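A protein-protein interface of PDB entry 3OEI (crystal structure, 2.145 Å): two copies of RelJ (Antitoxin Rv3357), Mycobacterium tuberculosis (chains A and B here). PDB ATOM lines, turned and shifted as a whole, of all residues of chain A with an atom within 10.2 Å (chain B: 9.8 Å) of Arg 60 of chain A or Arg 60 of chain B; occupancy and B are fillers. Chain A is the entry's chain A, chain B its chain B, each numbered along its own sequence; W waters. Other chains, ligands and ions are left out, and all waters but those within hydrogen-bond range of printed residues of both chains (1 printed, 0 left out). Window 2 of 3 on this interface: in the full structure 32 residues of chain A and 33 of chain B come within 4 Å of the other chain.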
ATOM      1  N   TYR A  51       9.897   3.715  31.827  1.00  0.00           N
ATOM      2  CA  TYR A  51      10.833   4.426  32.664  1.00  0.00           C
ATOM      3  C   TYR A  51      12.178   4.623  31.941  1.00  0.00           C
ATOM      4  O   TYR A  51      12.700   5.739  31.913  1.00  0.00           O
ATOM      5  CB  TYR A  51      11.018   3.715  34.012  1.00  0.00           C
ATOM      6  CG  TYR A  51      12.043   4.403  34.872  1.00  0.00           C
ATOM      7  CD1 TYR A  51      11.786   5.660  35.416  1.00  0.00           C
ATOM      8  CD2 TYR A  51      13.274   3.809  35.128  1.00  0.00           C
ATOM      9  CE1 TYR A  51      12.743   6.317  36.192  1.00  0.00           C
ATOM     10  CE2 TYR A  51      14.238   4.459  35.907  1.00  0.00           C
ATOM     11  CZ  TYR A  51      13.960   5.704  36.435  1.00  0.00           C
ATOM     12  OH  TYR A  51      14.905   6.356  37.209  1.00  0.00           O
ATOM     13  N   LEU A  52      12.711   3.566  31.328  1.00  0.00           N
ATOM     14  CA  LEU A  52      14.006   3.667  30.624  1.00  0.00           C
ATOM     15  C   LEU A  52      13.921   4.609  29.422  1.00  0.00           C
ATOM     16  O   LEU A  52      14.873   5.320  29.112  1.00  0.00           O
ATOM     17  CB  LEU A  52      14.516   2.290  30.189  1.00  0.00           C
ATOM     18  CG  LEU A  52      14.902   1.332  31.326  1.00  0.00           C
ATOM     19  CD1 LEU A  52      15.018  -0.118  30.848  1.00  0.00           C
ATOM     20  CD2 LEU A  52      16.181   1.771  32.022  1.00  0.00           C
ATOM     21  N   LEU A  53      12.762   4.642  28.770  1.00  0.00           N
ATOM     22  CA  LEU A  53      12.632   5.364  27.514  1.00  0.00           C
ATOM     23  C   LEU A  53      12.061   6.783  27.603  1.00  0.00           C
ATOM     24  O   LEU A  53      12.117   7.530  26.613  1.00  0.00           O
ATOM     25  CB  LEU A  53      11.848   4.528  26.501  1.00  0.00           C
ATOM     26  CG  LEU A  53      12.596   3.308  25.970  1.00  0.00           C
ATOM     27  CD1 LEU A  53      11.726   2.492  25.019  1.00  0.00           C
ATOM     28  CD2 LEU A  53      13.897   3.723  25.281  1.00  0.00           C
ATOM     29  N   ARG A  54      11.551   7.169  28.771  1.00  0.00           N
ATOM     30  CA  ARG A  54      10.812   8.436  28.923  1.00  0.00           C
ATOM     31  C   ARG A  54      11.705   9.683  29.055  1.00  0.00           C
ATOM     32  O   ARG A  54      11.247  10.800  28.858  1.00  0.00           O
ATOM     33  CB  ARG A  54       9.877   8.373  30.134  1.00  0.00           C
ATOM     34  CG  ARG A  54      10.622   8.351  31.449  1.00  0.00           C
ATOM     35  CD  ARG A  54       9.680   8.403  32.633  1.00  0.00           C
ATOM     36  NE  ARG A  54       9.157   9.748  32.859  1.00  0.00           N
ATOM     37  CZ  ARG A  54       8.216  10.035  33.757  1.00  0.00           C
ATOM     38  NH1 ARG A  54       7.696   9.059  34.494  1.00  0.00           N
ATOM     39  NH2 ARG A  54       7.788  11.289  33.911  1.00  0.00           N
ATOM     40  N   SER A  55      12.961   9.491  29.430  1.00  0.00           N
ATOM     41  CA  SER A  55      13.910  10.590  29.453  1.00  0.00           C
ATOM     42  C   SER A  55      14.627  10.564  28.118  1.00  0.00           C
ATOM     43  O   SER A  55      15.246   9.570  27.760  1.00  0.00           O
ATOM     44  CB  SER A  55      14.896  10.447  30.612  1.00  0.00           C
ATOM     45  OG  SER A  55      15.964  11.365  30.493  1.00  0.00           O
ATOM     46  N   PRO A  56      14.512  11.647  27.350  1.00  0.00           N
ATOM     47  CA  PRO A  56      15.020  11.540  25.979  1.00  0.00           C
ATOM     48  C   PRO A  56      16.517  11.237  25.953  1.00  0.00           C
ATOM     49  O   PRO A  56      16.961  10.449  25.109  1.00  0.00           O
ATOM     50  CB  PRO A  56      14.688  12.904  25.361  1.00  0.00           C
ATOM     51  CG  PRO A  56      14.336  13.793  26.496  1.00  0.00           C
ATOM     52  CD  PRO A  56      13.789  12.902  27.582  1.00  0.00           C
ATOM     53  N   GLU A  57      17.272  11.803  26.890  1.00  0.00           N
ATOM     54  CA  GLU A  57      18.704  11.532  26.956  1.00  0.00           C
ATOM     55  C   GLU A  57      18.964  10.062  27.284  1.00  0.00           C
ATOM     56  O   GLU A  57      19.840   9.422  26.689  1.00  0.00           O
ATOM     57  CB  GLU A  57      19.366  12.440  27.995  1.00  0.00           C
ATOM     58  CG  GLU A  57      20.883  12.274  28.087  1.00  0.00           C
ATOM     59  CD  GLU A  57      21.607  12.775  26.835  1.00  0.00           C
ATOM     60  OE1 GLU A  57      20.924  13.229  25.883  1.00  0.00           O
ATOM     61  OE2 GLU A  57      22.860  12.722  26.820  1.00  0.00           O
ATOM     62  N   ASN A  58      18.192   9.515  28.223  1.00  0.00           N
ATOM     63  CA  ASN A  58      18.380   8.121  28.596  1.00  0.00           C
ATOM     64  C   ASN A  58      17.962   7.191  27.473  1.00  0.00           C
ATOM     65  O   ASN A  58      18.627   6.195  27.228  1.00  0.00           O
ATOM     66  CB  ASN A  58      17.637   7.759  29.897  1.00  0.00           C
ATOM     67  CG  ASN A  58      18.167   6.477  30.521  1.00  0.00           C
ATOM     68  OD1 ASN A  58      19.200   6.499  31.187  1.00  0.00           O
ATOM     69  ND2 ASN A  58      17.482   5.349  30.282  1.00  0.00           N
ATOM     70  N   ALA A  59      16.846   7.505  26.804  1.00  0.00           N
ATOM     71  CA  ALA A  59      16.416   6.726  25.646  1.00  0.00           C
ATOM     72  C   ALA A  59      17.496   6.686  24.569  1.00  0.00           C
ATOM     73  O   ALA A  59      17.811   5.628  24.045  1.00  0.00           O
ATOM     74  CB  ALA A  59      15.090   7.265  25.058  1.00  0.00           C
ATOM     75  N   ARG A  60      18.058   7.842  24.238  1.00  0.00           N
ATOM     76  CA  ARG A  60      19.106   7.896  23.209  1.00  0.00           C
ATOM     77  C   ARG A  60      20.356   7.047  23.525  1.00  0.00           C
ATOM     78  O   ARG A  60      20.799   6.230  22.701  1.00  0.00           O
ATOM     79  CB  ARG A  60      19.508   9.354  22.950  1.00  0.00           C
ATOM     80  CG  ARG A  60      19.980   9.612  21.542  1.00  0.00           C
ATOM     81  CD  ARG A  60      21.405  10.115  21.543  1.00  0.00           C
ATOM     82  NE  ARG A  60      21.609  11.193  22.513  1.00  0.00           N
ATOM     83  CZ  ARG A  60      22.745  11.385  23.179  1.00  0.00           C
ATOM     84  NH1 ARG A  60      23.780  10.576  22.980  1.00  0.00           N
ATOM     85  NH2 ARG A  60      22.849  12.388  24.041  1.00  0.00           N
ATOM     86  N   ARG A  61      20.937   7.237  24.707  1.00  0.00           N
ATOM     87  CA  ARG A  61      22.117   6.446  25.082  1.00  0.00           C
ATOM     88  C   ARG A  61      21.786   4.958  25.073  1.00  0.00           C
ATOM     89  O   ARG A  61      22.551   4.142  24.558  1.00  0.00           O
ATOM     90  CB  ARG A  61      22.657   6.844  26.468  1.00  0.00           C
ATOM     91  CG  ARG A  61      22.915   8.334  26.661  1.00  0.00           C
ATOM     92  CD  ARG A  61      24.221   8.758  26.042  1.00  0.00           C
ATOM     93  NE  ARG A  61      25.375   8.176  26.739  1.00  0.00           N
ATOM     94  CZ  ARG A  61      26.040   8.771  27.726  1.00  0.00           C
ATOM     95  NH1 ARG A  61      25.679   9.980  28.143  1.00  0.00           N
ATOM     96  NH2 ARG A  61      27.070   8.159  28.299  1.00  0.00           N
ATOM     97  N   LEU A  62      20.637   4.596  25.638  1.00  0.00           N
ATOM     98  CA  LEU A  62      20.329   3.183  25.773  1.00  0.00           C
ATOM     99  C   LEU A  62      20.155   2.565  24.397  1.00  0.00           C
ATOM    100  O   LEU A  62      20.718   1.512  24.127  1.00  0.00           O
ATOM    101  CB  LEU A  62      19.077   2.966  26.640  1.00  0.00           C
ATOM    102  CG  LEU A  62      18.456   1.569  26.692  1.00  0.00           C
ATOM    103  CD1 LEU A  62      19.491   0.507  26.999  1.00  0.00           C
ATOM    104  CD2 LEU A  62      17.354   1.537  27.728  1.00  0.00           C
ATOM    105  N   MET A  63      19.381   3.218  23.521  1.00  0.00           N
ATOM    106  CA  MET A  63      19.082   2.610  22.212  1.00  0.00           C
ATOM    107  C   MET A  63      20.289   2.623  21.248  1.00  0.00           C
ATOM    108  O   MET A  63      20.378   1.782  20.355  1.00  0.00           O
ATOM    109  CB  MET A  63      17.802   3.195  21.570  1.00  0.00           C
ATOM    110  CG  MET A  63      16.545   3.077  22.463  1.00  0.00           C
ATOM    111  SD  MET A  63      16.279   1.377  23.037  1.00  0.00           S
ATOM    112  CE  MET A  63      16.061   0.526  21.476  1.00  0.00           C
ATOM    113  N   GLU A  64      21.204   3.574  21.438  1.00  0.00           N
ATOM    114  CA  GLU A  64      22.527   3.534  20.787  1.00  0.00           C
ATOM    115  C   GLU A  64      23.351   2.343  21.273  1.00  0.00           C
ATOM    116  O   GLU A  64      23.932   1.613  20.475  1.00  0.00           O
ATOM    117  CB  GLU A  64      23.301   4.831  21.043  1.00  0.00           C
ATOM    118  CG  GLU A  64      22.794   6.001  20.218  1.00  0.00           C
ATOM    119  CD  GLU A  64      23.776   7.153  20.191  1.00  0.00           C
ATOM    120  OE1 GLU A  64      24.815   7.037  19.497  1.00  0.00           O
ATOM    121  OE2 GLU A  64      23.520   8.162  20.879  1.00  0.00           O
ATOM    122  N   ALA A  65      23.384   2.128  22.586  1.00  0.00           N
ATOM    123  CA  ALA A  65      23.953   0.889  23.099  1.00  0.00           C
ATOM    124  C   ALA A  65      23.268  -0.316  22.459  1.00  0.00           C
ATOM    125  O   ALA A  65      23.931  -1.234  21.987  1.00  0.00           O
ATOM    126  CB  ALA A  65      23.852   0.816  24.611  1.00  0.00           C
ATOM    127  N   VAL A  66      21.942  -0.313  22.424  1.00  0.00           N
ATOM    128  CA  VAL A  66      21.237  -1.434  21.808  1.00  0.00           C
ATOM    129  C   VAL A  66      21.653  -1.665  20.346  1.00  0.00           C
ATOM    130  O   VAL A  66      21.891  -2.798  19.940  1.00  0.00           O
ATOM    131  CB  VAL A  66      19.694  -1.269  21.873  1.00  0.00           C
ATOM    132  CG1 VAL A  66      19.018  -2.339  21.022  1.00  0.00           C
ATOM    133  CG2 VAL A  66      19.199  -1.333  23.333  1.00  0.00           C
ATOM    134  N   ALA A  67      21.704  -0.596  19.556  1.00  0.00           N
ATOM    135  CA  ALA A  67      22.095  -0.706  18.152  1.00  0.00           C
ATOM    136  C   ALA A  67      23.508  -1.312  18.007  1.00  0.00           C
ATOM    137  O   ALA A  67      23.735  -2.214  17.202  1.00  0.00           O
ATOM    138  CB  ALA A  67      22.017   0.652  17.461  1.00  0.00           C
ATOM    139  N   ARG A  68      24.459  -0.844  18.799  1.00  0.00           N
ATOM    140  CA  ARG A  68      25.790  -1.412  18.668  1.00  0.00           C
ATOM    141  C   ARG A  68      25.831  -2.846  19.173  1.00  0.00           C
ATOM    142  O   ARG A  68      26.544  -3.678  18.628  1.00  0.00           O
ATOM    143  CB  ARG A  68      26.865  -0.511  19.270  1.00  0.00           C
ATOM    144  CG  ARG A  68      26.953  -0.482  20.759  1.00  0.00           C
ATOM    145  CD  ARG A  68      28.069   0.496  21.172  1.00  0.00           C
ATOM    146  NE  ARG A  68      27.728   1.865  20.828  1.00  0.00           N
ATOM    147  CZ  ARG A  68      27.235   2.761  21.679  1.00  0.00           C
ATOM    148  NH1 ARG A  68      27.038   2.464  22.959  1.00  0.00           N
ATOM    149  NH2 ARG A  68      26.937   3.973  21.244  1.00  0.00           N
ATOM    150  N   VAL B  50       6.856   7.229  24.072  1.00  0.00           N
ATOM    151  CA  VAL B  50       7.948   6.294  24.046  1.00  0.00           C
ATOM    152  C   VAL B  50       8.293   5.894  22.607  1.00  0.00           C
ATOM    153  O   VAL B  50       9.463   5.677  22.286  1.00  0.00           O
ATOM    154  CB  VAL B  50       7.592   5.084  24.931  1.00  0.00           C
ATOM    155  CG1 VAL B  50       7.926   3.766  24.242  1.00  0.00           C
ATOM    156  CG2 VAL B  50       8.254   5.228  26.289  1.00  0.00           C
ATOM    157  N   LEU B  52       8.147   7.987  20.101  1.00  0.00           N
ATOM    158  CA  LEU B  52       8.953   9.117  19.608  1.00  0.00           C
ATOM    159  C   LEU B  52      10.419   9.148  20.094  1.00  0.00           C
ATOM    160  O   LEU B  52      11.300   9.601  19.373  1.00  0.00           O
ATOM    161  CB  LEU B  52       8.279  10.457  19.920  1.00  0.00           C
ATOM    162  CG  LEU B  52       6.962  10.691  19.172  1.00  0.00           C
ATOM    163  CD1 LEU B  52       6.174  11.844  19.824  1.00  0.00           C
ATOM    164  CD2 LEU B  52       7.191  10.944  17.674  1.00  0.00           C
ATOM    165  N   LEU B  53      10.659   8.675  21.314  1.00  0.00           N
ATOM    166  CA  LEU B  53      11.984   8.707  21.924  1.00  0.00           C
ATOM    167  C   LEU B  53      12.838   7.469  21.669  1.00  0.00           C
ATOM    168  O   LEU B  53      14.040   7.497  21.914  1.00  0.00           O
ATOM    169  CB  LEU B  53      11.862   8.905  23.430  1.00  0.00           C
ATOM    170  CG  LEU B  53      11.109  10.183  23.743  1.00  0.00           C
ATOM    171  CD1 LEU B  53      10.994  10.380  25.231  1.00  0.00           C
ATOM    172  CD2 LEU B  53      11.847  11.347  23.074  1.00  0.00           C
ATOM    173  N   ARG B  54      12.236   6.392  21.180  1.00  0.00           N
ATOM    174  CA  ARG B  54      12.945   5.116  21.114  1.00  0.00           C
ATOM    175  C   ARG B  54      13.898   4.954  19.924  1.00  0.00           C
ATOM    176  O   ARG B  54      14.622   3.963  19.836  1.00  0.00           O
ATOM    177  CB  ARG B  54      11.956   3.967  21.139  1.00  0.00           C
ATOM    178  CG  ARG B  54      11.272   3.741  19.799  1.00  0.00           C
ATOM    179  CD  ARG B  54      10.189   2.686  19.938  1.00  0.00           C
ATOM    180  NE  ARG B  54       9.755   2.203  18.631  1.00  0.00           N
ATOM    181  CZ  ARG B  54       8.734   1.371  18.448  1.00  0.00           C
ATOM    182  NH1 ARG B  54       8.038   0.942  19.489  1.00  0.00           N
ATOM    183  NH2 ARG B  54       8.416   0.969  17.221  1.00  0.00           N
ATOM    184  N   SER B  55      13.875   5.913  19.003  1.00  0.00           N
ATOM    185  CA  SER B  55      14.911   6.006  17.979  1.00  0.00           C
ATOM    186  C   SER B  55      15.816   7.154  18.362  1.00  0.00           C
ATOM    187  O   SER B  55      15.345   8.278  18.516  1.00  0.00           O
ATOM    188  CB  SER B  55      14.318   6.269  16.593  1.00  0.00           C
ATOM    189  OG  SER B  55      15.262   6.958  15.784  1.00  0.00           O
ATOM    190  N   PRO B  56      17.121   6.873  18.540  1.00  0.00           N
ATOM    191  CA  PRO B  56      18.088   7.889  18.983  1.00  0.00           C
ATOM    192  C   PRO B  56      18.101   9.124  18.082  1.00  0.00           C
ATOM    193  O   PRO B  56      18.140  10.251  18.569  1.00  0.00           O
ATOM    194  CB  PRO B  56      19.444   7.162  18.903  1.00  0.00           C
ATOM    195  CG  PRO B  56      19.131   5.708  19.019  1.00  0.00           C
ATOM    196  CD  PRO B  56      17.722   5.529  18.423  1.00  0.00           C
ATOM    197  N   GLU B  57      18.067   8.921  16.772  1.00  0.00           N
ATOM    198  CA  GLU B  57      18.087  10.064  15.869  1.00  0.00           C
ATOM    199  C   GLU B  57      16.782  10.853  15.970  1.00  0.00           C
ATOM    200  O   GLU B  57      16.783  12.082  15.859  1.00  0.00           O
ATOM    201  CB  GLU B  57      18.359   9.624  14.432  1.00  0.00           C
ATOM    202  CG  GLU B  57      18.667  10.771  13.478  1.00  0.00           C
ATOM    203  CD  GLU B  57      19.748  11.706  14.008  1.00  0.00           C
ATOM    204  OE1 GLU B  57      20.799  11.209  14.490  1.00  0.00           O
ATOM    205  OE2 GLU B  57      19.540  12.940  13.949  1.00  0.00           O
ATOM    206  N   ASN B  58      15.664  10.169  16.220  1.00  0.00           N
ATOM    207  CA  ASN B  58      14.407  10.904  16.316  1.00  0.00           C
ATOM    208  C   ASN B  58      14.360  11.708  17.578  1.00  0.00           C
ATOM    209  O   ASN B  58      13.923  12.848  17.578  1.00  0.00           O
ATOM    210  CB  ASN B  58      13.176   9.988  16.256  1.00  0.00           C
ATOM    211  CG  ASN B  58      11.945  10.738  15.829  1.00  0.00           C
ATOM    212  OD1 ASN B  58      11.846  11.164  14.673  1.00  0.00           O
ATOM    213  ND2 ASN B  58      11.005  10.940  16.762  1.00  0.00           N
ATOM    214  N   ALA B  59      14.827  11.099  18.658  1.00  0.00           N
ATOM    215  CA  ALA B  59      14.797  11.731  19.966  1.00  0.00           C
ATOM    216  C   ALA B  59      15.627  12.991  19.884  1.00  0.00           C
ATOM    217  O   ALA B  59      15.242  14.051  20.389  1.00  0.00           O
ATOM    218  CB  ALA B  59      15.373  10.774  21.026  1.00  0.00           C
ATOM    219  N   ARG B  60      16.781  12.867  19.240  1.00  0.00           N
ATOM    220  CA  ARG B  60      17.677  14.003  19.079  1.00  0.00           C
ATOM    221  C   ARG B  60      17.026  15.140  18.294  1.00  0.00           C
ATOM    222  O   ARG B  60      17.008  16.287  18.737  1.00  0.00           O
ATOM    223  CB  ARG B  60      18.977  13.573  18.393  1.00  0.00           C
ATOM    224  CG  ARG B  60      19.847  14.760  17.976  1.00  0.00           C
ATOM    225  CD  ARG B  60      21.235  14.316  17.573  1.00  0.00           C
ATOM    226  NE  ARG B  60      21.869  13.532  18.635  1.00  0.00           N
ATOM    227  CZ  ARG B  60      22.453  14.055  19.712  1.00  0.00           C
ATOM    228  NH1 ARG B  60      22.482  15.371  19.891  1.00  0.00           N
ATOM    229  NH2 ARG B  60      23.011  13.263  20.616  1.00  0.00           N
ATOM    230  N   ARG B  61      16.484  14.824  17.123  1.00  0.00           N
ATOM    231  CA  ARG B  61      15.879  15.856  16.283  1.00  0.00           C
ATOM    232  C   ARG B  61      14.697  16.533  16.989  1.00  0.00           C
ATOM    233  O   ARG B  61      14.460  17.735  16.835  1.00  0.00           O
ATOM    234  CB  ARG B  61      15.428  15.258  14.949  1.00  0.00           C
ATOM    235  CG  ARG B  61      16.547  14.994  13.954  1.00  0.00           C
ATOM    236  CD  ARG B  61      16.977  16.297  13.309  1.00  0.00           C
ATOM    237  NE  ARG B  61      17.375  16.130  11.911  1.00  0.00           N
ATOM    238  CZ  ARG B  61      16.563  16.314  10.871  1.00  0.00           C
ATOM    239  NH1 ARG B  61      15.295  16.662  11.059  1.00  0.00           N
ATOM    240  NH2 ARG B  61      17.016  16.144   9.636  1.00  0.00           N
ATOM    241  N   LEU B  62      13.969  15.764  17.779  1.00  0.00           N
ATOM    242  CA  LEU B  62      12.743  16.268  18.403  1.00  0.00           C
ATOM    243  C   LEU B  62      13.041  17.213  19.551  1.00  0.00           C
ATOM    244  O   LEU B  62      12.423  18.273  19.674  1.00  0.00           O
ATOM    245  CB  LEU B  62      11.879  15.105  18.914  1.00  0.00           C
ATOM    246  CG  LEU B  62      10.618  15.461  19.712  1.00  0.00           C
ATOM    247  CD1 LEU B  62       9.754  16.535  19.024  1.00  0.00           C
ATOM    248  CD2 LEU B  62       9.817  14.194  19.927  1.00  0.00           C
ATOM    249  N   MET B  63      13.977  16.819  20.411  1.00  0.00           N
ATOM    250  CA  MET B  63      14.338  17.658  21.549  1.00  0.00           C
ATOM    251  C   MET B  63      15.054  18.946  21.071  1.00  0.00           C
ATOM    252  O   MET B  63      14.853  20.023  21.631  1.00  0.00           O
ATOM    253  CB  MET B  63      15.164  16.864  22.573  1.00  0.00           C
ATOM    254  CG  MET B  63      14.425  15.643  23.130  1.00  0.00           C
ATOM    255  SD  MET B  63      12.705  16.034  23.544  1.00  0.00           S
ATOM    256  CE  MET B  63      11.989  14.405  23.754  1.00  0.00           C
ATOM    257  N   GLU B  64      15.842  18.844  20.009  1.00  0.00           N
ATOM    258  CA  GLU B  64      16.383  20.057  19.401  1.00  0.00           C
ATOM    259  C   GLU B  64      15.248  21.009  18.998  1.00  0.00           C
ATOM    260  O   GLU B  64      15.277  22.199  19.334  1.00  0.00           O
ATOM    261  CB  GLU B  64      17.311  19.733  18.223  1.00  0.00           C
ATOM    262  CG  GLU B  64      18.640  19.086  18.662  1.00  0.00           C
ATOM    263  CD  GLU B  64      19.586  18.823  17.494  1.00  0.00           C
ATOM    264  OE1 GLU B  64      19.380  19.425  16.418  1.00  0.00           O
ATOM    265  OE2 GLU B  64      20.538  18.016  17.653  1.00  0.00           O
ATOM    266  N   ALA B  65      14.233  20.491  18.308  1.00  0.00           N
ATOM    267  CA  ALA B  65      13.066  21.317  17.996  1.00  0.00           C
ATOM    268  C   ALA B  65      12.376  21.827  19.259  1.00  0.00           C
ATOM    269  O   ALA B  65      11.900  22.968  19.306  1.00  0.00           O
ATOM    270  CB  ALA B  65      12.067  20.556  17.091  1.00  0.00           C
ATOM    271  N   VAL B  66      12.288  20.976  20.280  1.00  0.00           N
ATOM    272  CA  VAL B  66      11.617  21.382  21.518  1.00  0.00           C
ATOM    273  C   VAL B  66      12.392  22.495  22.231  1.00  0.00           C
ATOM    274  O   VAL B  66      11.797  23.432  22.784  1.00  0.00           O
ATOM    275  CB  VAL B  66      11.423  20.223  22.502  1.00  0.00           C
ATOM    276  CG1 VAL B  66      10.884  20.756  23.818  1.00  0.00           C
ATOM    277  CG2 VAL B  66      10.491  19.161  21.914  1.00  0.00           C
ATOM    278  N   ALA B  67      13.716  22.369  22.223  1.00  0.00           N
ATOM    279  CA  ALA B  67      14.593  23.377  22.817  1.00  0.00           C
ATOM    280  C   ALA B  67      14.432  24.739  22.125  1.00  0.00           C
ATOM    281  O   ALA B  67      14.275  25.755  22.790  1.00  0.00           O
ATOM    282  CB  ALA B  67      16.058  22.905  22.793  1.00  0.00           C
ATOM    283  N   ARG B  68      14.423  24.743  20.794  1.00  0.00           N
ATOM    284  CA  ARG B  68      14.218  25.977  20.030  1.00  0.00           C
ATOM    285  C   ARG B  68      12.886  26.605  20.361  1.00  0.00           C
ATOM    286  O   ARG B  68      12.783  27.811  20.539  1.00  0.00           O
ATOM    287  CB  ARG B  68      14.278  25.708  18.526  1.00  0.00           C
ATOM    288  CG  ARG B  68      15.676  25.509  17.987  1.00  0.00           C
ATOM    289  CD  ARG B  68      15.692  25.476  16.465  1.00  0.00           C
ATOM    290  NE  ARG B  68      14.979  24.325  15.922  1.00  0.00           N
ATOM    291  CZ  ARG B  68      15.548  23.147  15.679  1.00  0.00           C
ATOM    292  NH1 ARG B  68      16.837  22.971  15.948  1.00  0.00           N
ATOM    293  NH2 ARG B  68      14.828  22.145  15.183  1.00  0.00           N
HETATM  294  O   HOH W   1      16.481   6.672  21.560  1.00  0.00           O
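The guanidinium group of Arg 60 of chain B sits close to the guanidinium group of Arg 60 of chain A, 3.1 Å away.
Of the printed residues of chain B, Leu 53 of chain A touches Val 50 and Leu 53. Glu 57 of chain A touches none of the printed residues of chain B. Of chain B, only Leu 53 (3.3 Å) comes within 4 Å of Ala 59 of chain A. Arg 61 of chain A touches none of the printed residues of chain B. Of the printed residues of chain B, Met 63 of chain A touches Arg 54 (3.4 Å) and Pro 56 (3.8 Å). Of the printed residues of chain B, Glu 64 of chain A touches Pro 56 (3.8 Å). Of the printed residues of chain A, Leu 53 of chain B touches Leu 53 (3.4 Å), Arg 54 (3.7 Å), Pro 56 (3.97 Å) and Ala 59 (3.3 Å). Of the printed residues of chain A, Pro 56 of chain B touches Arg 60, Met 63 and Glu 64. Arg 60 of chain B touches just one residue of chain A: Arg 60 (3.1 Å). Of the printed residues of chain A, Met 63 of chain B touches Pro 56. Arg 68 of chain B touches none of the printed residues of chain A. The nearest residue of chain B that does not touch Arg 60 of chain A is Leu 53 of chain B (4.7 Å).
The guanidinium group (NH2) of Arg 60 of chain A lies within salt-bridge range of the side-chain carboxylate (OE1) of Glu 57 of chain A (2.8 Å). NH1 of Arg 60 of chain A lies within salt-bridge range of OE2 of Glu 64 of chain A. The guanidinium group (NH1) of Arg 60 of chain B lies within salt-bridge range of the side-chain carboxylate (OE2) of Glu 64 of chain B (3.97 Å).
Printed residues of chain B that touch a printed residue of chain A: Val 50, Leu 53, Arg 54, Pro 56, Arg 60 and Met 63. Hydrophobic or aromatic side chains of chain B that line the printed part of chain A: Val 50, Leu 53, Pro 56 and Met 63. Along chain B the printed residues that touch a printed residue of chain A span positions 50 to 63. Hydrophobic or aromatic side chains of chain A within 4 Å of the printed part of chain B: Leu 53, Pro 56, Ala 59 and Met 63. Among the printed residues, 11 pairs touch across the chains. Among the printed residues, no Asp or Glu carboxylate lies within 4 Å of a Lys or Arg side-chain nitrogen of the other chain.
Among the printed residues, pairs that only touch across the chains: Ala 59 of chain A with Leu 53 of chain B (3.3 Å), Leu 53 of chain A with Leu 53 of chain B (3.4 Å), Met 63 of chain A with Arg 54 of chain B (3.4 Å), Pro 56 of chain A with Met 63 of chain B (3.5 Å), Arg 60 of chain A with Pro 56 of chain B (3.6 Å), Arg 54 of chain A with Leu 53 of chain B (3.7 Å), Leu 53 of chain A with Val 50 of chain B (3.7 Å), Glu 64 of chain A with Pro 56 of chain B (3.8 Å), Met 63 of chain A with Pro 56 of chain B (3.8 Å) and Pro 56 of chain A with Leu 53 of chain B (3.97 Å).
Water W1 lies within hydrogen-bond range of the backbone carbonyl oxygen (O) of Leu 53 of chain B (2.6 Å), the backbone carbonyl oxygen (O) of Ala 59 of chain A (3.0 Å) and the backbone NH (N) of Arg 60 of chain A (3.3 Å).
Leu 53 of chain B touches its own counterpart, Leu 53 of chain A. Ala 59 of chain A touches Leu 53 of chain B, but with the chains exchanged Leu 53 of chain A does not touch Ala 59 of chain B (7.2 Å). Arg 60 of chain A touches Pro 56 of chain B, but with the chains exchanged Pro 56 of chain A does not touch Arg 60 of chain B (6.4 Å). Met 63 of chain A touches Arg 54 of chain B, but with the chains exchanged Arg 54 of chain A does not touch Met 63 of chain B (6.3 Å).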
